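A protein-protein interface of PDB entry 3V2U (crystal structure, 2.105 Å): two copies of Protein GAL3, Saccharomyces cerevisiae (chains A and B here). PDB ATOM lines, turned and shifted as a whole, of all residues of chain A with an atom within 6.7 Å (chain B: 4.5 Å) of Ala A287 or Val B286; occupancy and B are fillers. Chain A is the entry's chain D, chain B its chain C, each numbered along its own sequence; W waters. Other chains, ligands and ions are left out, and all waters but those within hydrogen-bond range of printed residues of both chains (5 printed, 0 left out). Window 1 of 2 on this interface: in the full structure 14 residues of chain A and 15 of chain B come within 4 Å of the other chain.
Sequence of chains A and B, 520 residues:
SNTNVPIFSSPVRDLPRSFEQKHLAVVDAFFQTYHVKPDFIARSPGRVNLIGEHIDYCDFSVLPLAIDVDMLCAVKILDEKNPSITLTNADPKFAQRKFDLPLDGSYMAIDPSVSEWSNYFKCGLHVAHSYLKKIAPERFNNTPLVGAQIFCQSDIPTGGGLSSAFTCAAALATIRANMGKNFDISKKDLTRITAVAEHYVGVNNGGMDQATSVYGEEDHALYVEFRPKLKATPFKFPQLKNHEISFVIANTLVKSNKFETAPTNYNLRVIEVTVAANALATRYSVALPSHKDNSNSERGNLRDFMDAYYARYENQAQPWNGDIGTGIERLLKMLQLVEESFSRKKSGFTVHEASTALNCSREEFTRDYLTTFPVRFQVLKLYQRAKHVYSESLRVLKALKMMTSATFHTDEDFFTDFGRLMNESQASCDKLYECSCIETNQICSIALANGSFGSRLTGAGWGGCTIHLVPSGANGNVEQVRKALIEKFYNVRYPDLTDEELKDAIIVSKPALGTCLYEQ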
ATOM      1  N   ALA A 281      12.236  -0.845  15.298  1.00  0.00           N
ATOM      2  CA  ALA A 281      13.095  -0.056  16.166  1.00  0.00           C
ATOM      3  C   ALA A 281      12.297   1.042  16.857  1.00  0.00           C
ATOM      4  O   ALA A 281      12.485   1.301  18.051  1.00  0.00           O
ATOM      5  CB  ALA A 281      14.251   0.551  15.370  1.00  0.00           C
ATOM      6  N   SER A 285      11.570   1.259  20.887  1.00  0.00           N
ATOM      7  CA  SER A 285      12.383   2.330  21.440  1.00  0.00           C
ATOM      8  C   SER A 285      13.878   2.019  21.439  1.00  0.00           C
ATOM      9  O   SER A 285      14.551   2.193  22.452  1.00  0.00           O
ATOM     10  CB  SER A 285      11.925   2.662  22.863  1.00  0.00           C
ATOM     11  OG  SER A 285      10.604   3.163  22.842  1.00  0.00           O
ATOM     12  N   VAL A 286      14.392   1.559  20.304  1.00  0.00           N
ATOM     13  CA  VAL A 286      15.835   1.456  20.124  1.00  0.00           C
ATOM     14  C   VAL A 286      16.237   2.222  18.871  1.00  0.00           C
ATOM     15  O   VAL A 286      15.420   2.441  17.986  1.00  0.00           O
ATOM     16  CB  VAL A 286      16.304  -0.004  20.004  1.00  0.00           C
ATOM     17  CG1 VAL A 286      16.135  -0.741  21.349  1.00  0.00           C
ATOM     18  CG2 VAL A 286      15.562  -0.714  18.884  1.00  0.00           C
ATOM     19  N   ALA A 287      17.493   2.637  18.800  1.00  0.00           N
ATOM     20  CA  ALA A 287      17.982   3.335  17.617  1.00  0.00           C
ATOM     21  C   ALA A 287      18.794   2.358  16.789  1.00  0.00           C
ATOM     22  O   ALA A 287      19.350   1.412  17.331  1.00  0.00           O
ATOM     23  CB  ALA A 287      18.825   4.545  18.027  1.00  0.00           C
ATOM     24  N   LEU A 288      18.821   2.549  15.475  1.00  0.00           N
ATOM     25  CA  LEU A 288      19.636   1.709  14.585  1.00  0.00           C
ATOM     26  C   LEU A 288      20.829   2.513  14.078  1.00  0.00           C
ATOM     27  O   LEU A 288      20.761   3.739  14.016  1.00  0.00           O
ATOM     28  CB  LEU A 288      18.825   1.242  13.382  1.00  0.00           C
ATOM     29  CG  LEU A 288      17.551   0.455  13.657  1.00  0.00           C
ATOM     30  CD1 LEU A 288      16.985  -0.022  12.325  1.00  0.00           C
ATOM     31  CD2 LEU A 288      17.843  -0.721  14.585  1.00  0.00           C
ATOM     32  N   PRO A 289      21.919   1.826  13.704  1.00  0.00           N
ATOM     33  CA  PRO A 289      23.066   2.551  13.146  1.00  0.00           C
ATOM     34  C   PRO A 289      22.699   3.183  11.808  1.00  0.00           C
ATOM     35  O   PRO A 289      21.750   2.734  11.155  1.00  0.00           O
ATOM     36  CB  PRO A 289      24.114   1.451  12.949  1.00  0.00           C
ATOM     37  CG  PRO A 289      23.306   0.191  12.788  1.00  0.00           C
ATOM     38  CD  PRO A 289      22.108   0.364  13.674  1.00  0.00           C
ATOM     39  N   ASP A 304      20.480  -5.290  12.253  1.00  0.00           N
ATOM     40  CA  ASP A 304      20.753  -4.158  13.129  1.00  0.00           C
ATOM     41  C   ASP A 304      19.661  -4.089  14.196  1.00  0.00           C
ATOM     42  O   ASP A 304      19.958  -3.813  15.361  1.00  0.00           O
ATOM     43  CB  ASP A 304      20.802  -2.839  12.347  1.00  0.00           C
ATOM     44  CG  ASP A 304      21.963  -2.768  11.352  1.00  0.00           C
ATOM     45  OD1 ASP A 304      23.067  -3.288  11.623  1.00  0.00           O
ATOM     46  OD2 ASP A 304      21.771  -2.157  10.287  1.00  0.00           O
ATOM     47  N   PHE A 305      18.406  -4.356  13.811  1.00  0.00           N
ATOM     48  CA  PHE A 305      17.328  -4.342  14.802  1.00  0.00           C
ATOM     49  C   PHE A 305      17.480  -5.463  15.818  1.00  0.00           C
ATOM     50  O   PHE A 305      17.295  -5.256  17.013  1.00  0.00           O
ATOM     51  CB  PHE A 305      15.916  -4.406  14.203  1.00  0.00           C
ATOM     52  CG  PHE A 305      14.856  -4.541  15.264  1.00  0.00           C
ATOM     53  CD1 PHE A 305      14.588  -3.476  16.128  1.00  0.00           C
ATOM     54  CD2 PHE A 305      14.210  -5.748  15.480  1.00  0.00           C
ATOM     55  CE1 PHE A 305      13.646  -3.601  17.163  1.00  0.00           C
ATOM     56  CE2 PHE A 305      13.270  -5.888  16.506  1.00  0.00           C
ATOM     57  CZ  PHE A 305      12.984  -4.809  17.349  1.00  0.00           C
ATOM     58  N   ALA A 308      20.183  -4.345  18.136  1.00  0.00           N
ATOM     59  CA  ALA A 308      19.758  -3.208  18.957  1.00  0.00           C
ATOM     60  C   ALA A 308      18.773  -3.637  20.045  1.00  0.00           C
ATOM     61  O   ALA A 308      18.874  -3.195  21.192  1.00  0.00           O
ATOM     62  CB  ALA A 308      19.139  -2.108  18.084  1.00  0.00           C
ATOM     63  N   TYR A 309      17.800  -4.467  19.665  1.00  0.00           N
ATOM     64  CA  TYR A 309      16.830  -4.992  20.617  1.00  0.00           C
ATOM     65  C   TYR A 309      17.535  -5.728  21.755  1.00  0.00           C
ATOM     66  O   TYR A 309      17.226  -5.532  22.930  1.00  0.00           O
ATOM     67  CB  TYR A 309      15.826  -5.935  19.941  1.00  0.00           C
ATOM     68  CG  TYR A 309      14.807  -6.458  20.923  1.00  0.00           C
ATOM     69  CD1 TYR A 309      13.596  -5.792  21.121  1.00  0.00           C
ATOM     70  CD2 TYR A 309      15.072  -7.598  21.694  1.00  0.00           C
ATOM     71  CE1 TYR A 309      12.655  -6.257  22.063  1.00  0.00           C
ATOM     72  CE2 TYR A 309      14.140  -8.068  22.627  1.00  0.00           C
ATOM     73  CZ  TYR A 309      12.936  -7.398  22.803  1.00  0.00           C
ATOM     74  OH  TYR A 309      12.022  -7.864  23.725  1.00  0.00           O
ATOM     75  N   ARG A 312      19.578  -3.597  24.271  1.00  0.00           N
ATOM     76  CA  ARG A 312      18.734  -2.797  25.148  1.00  0.00           C
ATOM     77  C   ARG A 312      18.049  -3.651  26.218  1.00  0.00           C
ATOM     78  O   ARG A 312      17.946  -3.235  27.381  1.00  0.00           O
ATOM     79  CB  ARG A 312      17.689  -2.030  24.322  1.00  0.00           C
ATOM     80  CG  ARG A 312      16.592  -1.341  25.143  1.00  0.00           C
ATOM     81  CD  ARG A 312      17.167  -0.320  26.120  1.00  0.00           C
ATOM     82  NE  ARG A 312      16.101   0.391  26.833  1.00  0.00           N
ATOM     83  CZ  ARG A 312      15.497  -0.064  27.931  1.00  0.00           C
ATOM     84  NH1 ARG A 312      15.850  -1.233  28.463  1.00  0.00           N
ATOM     85  NH2 ARG A 312      14.539   0.650  28.498  1.00  0.00           N
ATOM     86  N   ALA B 281      20.726  11.859  22.308  1.00  0.00           N
ATOM     87  CA  ALA B 281      20.147  10.544  22.027  1.00  0.00           C
ATOM     88  C   ALA B 281      20.607  10.020  20.669  1.00  0.00           C
ATOM     89  O   ALA B 281      20.912   8.842  20.531  1.00  0.00           O
ATOM     90  CB  ALA B 281      18.627  10.601  22.073  1.00  0.00           C
ATOM     91  N   TYR B 284      24.346   8.967  20.720  1.00  0.00           N
ATOM     92  CA  TYR B 284      24.610   7.735  21.474  1.00  0.00           C
ATOM     93  C   TYR B 284      23.669   6.581  21.113  1.00  0.00           C
ATOM     94  O   TYR B 284      23.587   5.595  21.844  1.00  0.00           O
ATOM     95  CB  TYR B 284      24.585   8.016  22.984  1.00  0.00           C
ATOM     96  CG  TYR B 284      25.741   8.885  23.413  1.00  0.00           C
ATOM     97  CD1 TYR B 284      27.024   8.356  23.552  1.00  0.00           C
ATOM     98  CD2 TYR B 284      25.563  10.244  23.640  1.00  0.00           C
ATOM     99  CE1 TYR B 284      28.094   9.165  23.918  1.00  0.00           C
ATOM    100  CE2 TYR B 284      26.615  11.053  24.017  1.00  0.00           C
ATOM    101  CZ  TYR B 284      27.875  10.518  24.150  1.00  0.00           C
ATOM    102  OH  TYR B 284      28.911  11.348  24.515  1.00  0.00           O
ATOM    103  N   SER B 285      22.969   6.713  19.987  1.00  0.00           N
ATOM    104  CA  SER B 285      22.045   5.682  19.509  1.00  0.00           C
ATOM    105  C   SER B 285      21.059   5.132  20.550  1.00  0.00           C
ATOM    106  O   SER B 285      20.998   3.931  20.787  1.00  0.00           O
ATOM    107  CB  SER B 285      22.809   4.509  18.868  1.00  0.00           C
ATOM    108  OG  SER B 285      23.697   4.964  17.876  1.00  0.00           O
ATOM    109  N   VAL B 286      20.280   6.011  21.163  1.00  0.00           N
ATOM    110  CA  VAL B 286      19.182   5.557  21.999  1.00  0.00           C
ATOM    111  C   VAL B 286      17.940   6.317  21.593  1.00  0.00           C
ATOM    112  O   VAL B 286      18.033   7.402  21.031  1.00  0.00           O
ATOM    113  CB  VAL B 286      19.448   5.765  23.513  1.00  0.00           C
ATOM    114  CG1 VAL B 286      20.611   4.893  23.977  1.00  0.00           C
ATOM    115  CG2 VAL B 286      19.707   7.236  23.835  1.00  0.00           C
ATOM    116  N   ALA B 287      16.783   5.734  21.884  1.00  0.00           N
ATOM    117  CA  ALA B 287      15.501   6.352  21.589  1.00  0.00           C
ATOM    118  C   ALA B 287      14.963   6.984  22.863  1.00  0.00           C
ATOM    119  O   ALA B 287      15.180   6.448  23.945  1.00  0.00           O
ATOM    120  CB  ALA B 287      14.531   5.290  21.074  1.00  0.00           C
ATOM    121  N   LEU B 288      14.301   8.131  22.741  1.00  0.00           N
ATOM    122  CA  LEU B 288      13.617   8.758  23.885  1.00  0.00           C
ATOM    123  C   LEU B 288      12.114   8.496  23.790  1.00  0.00           C
ATOM    124  O   LEU B 288      11.600   8.265  22.695  1.00  0.00           O
ATOM    125  CB  LEU B 288      13.878  10.265  23.919  1.00  0.00           C
ATOM    126  CG  LEU B 288      15.331  10.732  23.906  1.00  0.00           C
ATOM    127  CD1 LEU B 288      15.381  12.246  23.999  1.00  0.00           C
ATOM    128  CD2 LEU B 288      16.129  10.089  25.057  1.00  0.00           C
ATOM    129  N   PHE B 305      16.937  11.277  28.470  1.00  0.00           N
ATOM    130  CA  PHE B 305      18.196  10.825  27.880  1.00  0.00           C
ATOM    131  C   PHE B 305      19.036  10.096  28.928  1.00  0.00           C
ATOM    132  O   PHE B 305      19.593   9.037  28.655  1.00  0.00           O
ATOM    133  CB  PHE B 305      19.016  11.958  27.251  1.00  0.00           C
ATOM    134  CG  PHE B 305      20.411  11.521  26.869  1.00  0.00           C
ATOM    135  CD1 PHE B 305      20.612  10.678  25.776  1.00  0.00           C
ATOM    136  CD2 PHE B 305      21.509  11.901  27.629  1.00  0.00           C
ATOM    137  CE1 PHE B 305      21.893  10.227  25.440  1.00  0.00           C
ATOM    138  CE2 PHE B 305      22.794  11.469  27.296  1.00  0.00           C
ATOM    139  CZ  PHE B 305      22.984  10.626  26.198  1.00  0.00           C
ATOM    140  N   ALA B 308      17.648   6.703  29.376  1.00  0.00           N
ATOM    141  CA  ALA B 308      17.825   5.876  28.190  1.00  0.00           C
ATOM    142  C   ALA B 308      19.292   5.496  27.996  1.00  0.00           C
ATOM    143  O   ALA B 308      19.592   4.402  27.551  1.00  0.00           O
ATOM    144  CB  ALA B 308      17.261   6.591  26.939  1.00  0.00           C
ATOM    145  N   ARG B 312      20.731   1.499  28.337  1.00  0.00           N
ATOM    146  CA  ARG B 312      21.427   0.922  27.189  1.00  0.00           C
ATOM    147  C   ARG B 312      22.890   0.555  27.461  1.00  0.00           C
ATOM    148  O   ARG B 312      23.358  -0.499  27.033  1.00  0.00           O
ATOM    149  CB  ARG B 312      21.344   1.879  25.997  1.00  0.00           C
ATOM    150  CG  ARG B 312      22.249   1.510  24.814  1.00  0.00           C
ATOM    151  CD  ARG B 312      21.938   0.130  24.257  1.00  0.00           C
ATOM    152  NE  ARG B 312      22.800  -0.202  23.120  1.00  0.00           N
ATOM    153  CZ  ARG B 312      23.987  -0.792  23.224  1.00  0.00           C
ATOM    154  NH1 ARG B 312      24.466  -1.133  24.414  1.00  0.00           N
ATOM    155  NH2 ARG B 312      24.698  -1.047  22.131  1.00  0.00           N
ATOM    156  N   TYR B 313      23.613   1.436  28.145  1.00  0.00           N
ATOM    157  CA  TYR B 313      25.049   1.237  28.366  1.00  0.00           C
ATOM    158  C   TYR B 313      25.449   0.889  29.811  1.00  0.00           C
ATOM    159  O   TYR B 313      26.585   0.490  30.070  1.00  0.00           O
ATOM    160  CB  TYR B 313      25.819   2.476  27.904  1.00  0.00           C
ATOM    161  CG  TYR B 313      25.610   2.791  26.440  1.00  0.00           C
ATOM    162  CD1 TYR B 313      26.148   1.977  25.455  1.00  0.00           C
ATOM    163  CD2 TYR B 313      24.852   3.886  26.047  1.00  0.00           C
ATOM    164  CE1 TYR B 313      25.948   2.253  24.108  1.00  0.00           C
ATOM    165  CE2 TYR B 313      24.645   4.174  24.715  1.00  0.00           C
ATOM    166  CZ  TYR B 313      25.199   3.353  23.745  1.00  0.00           C
ATOM    167  OH  TYR B 313      24.996   3.644  22.415  1.00  0.00           O
HETATM  168  O   HOH W   1      22.002   5.970  15.139  1.00  0.00           O
HETATM  169  O   HOH W   2      17.182   2.929  23.323  1.00  0.00           O
HETATM  170  O   HOH W   3      17.728   3.041  25.938  1.00  0.00           O
HETATM  171  O   HOH W   4      19.132   1.824  21.247  1.00  0.00           O
HETATM  172  O   HOH W   5      19.949  -0.622  21.470  1.00  0.00           O
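The backbone carbonyl oxygen (O) of Ala B281 is in hydrogen-bond range of the backbone NH (N) of Val B286, at 3.0 Å. O of Ala A281 sits at hydrogen-bond distance from N of Val A286 (3.0 Å).
Ser A285 touches Ala B287. Ala B287 touches Val A286 (CB to N, 3.8 Å). Ser B285 touches Ala A287 (C to CB, 3.4 Å). Ala A287 touches Val B286.
Of the printed residues of chain B, Ala A287 touches Ser B285 (3.4 Å) and Val B286 (3.8 Å). Of chain A, only Ala A287 comes within 4 Å of Val B286. Printed residues of chain B within 4 Å of Val A286: Ala B287. Of the printed residues of chain A, Ala B287 touches Ser A285 (3.4 Å) and Val A286 (3.8 Å). Printed residues of chain B within 4 Å of Ser A285: Ala B287. Of the printed residues of chain A, Ser B285 touches Ala A287. Leu B288 touches none of the printed residues of chain A. Pro A289 touches none of the printed residues of chain B. The nearest printed residue of chain B that does not touch Ser A285 is Leu B288 (5.2 Å).
Of the 11 printed residues of chain A, 3 touch a printed residue of chain B. Hydrophobic or aromatic side chains of chain A within 4 Å of the printed part of chain B: Ala A287. Printed residues of chain B that touch a printed residue of chain A: Ser B285, Val B286 and Ala B287. Among the printed residues, 4 pairs touch across the chains. Among the printed residues, no Asp or Glu carboxylate lies within 4 Å of a Lys or Arg side-chain nitrogen of the other chain.
Ser A285 touches Ala B287, and with the chains exchanged Ala A287 touches Ser B285. Val A286 touches Ala B287, and with the chains exchanged Ala A287 touches Val B286.
Water W1 bridges the backbone carbonyl oxygen (O) of Leu A288 (2.8 Å) and the side-chain hydroxyl (OG) of Ser B285 (3.4 Å). Water W5 lies within hydrogen-bond range of O of Ala A308 and NE of Arg B312. Water W3 bridges the backbone carbonyl oxygen of Ala B308 (2.8 Å) and the guanidinium group of Arg A312 (3.2 Å). Water W4 lies within hydrogen-bond range of the backbone carbonyl oxygen of Ser B285 (2.9 Å) and the backbone NH of Ala A287 (3.1 Å). Water W2 bridges the backbone carbonyl oxygen of Ser A285 (2.9 Å) and the backbone NH of Ala B287 (3.2 Å).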
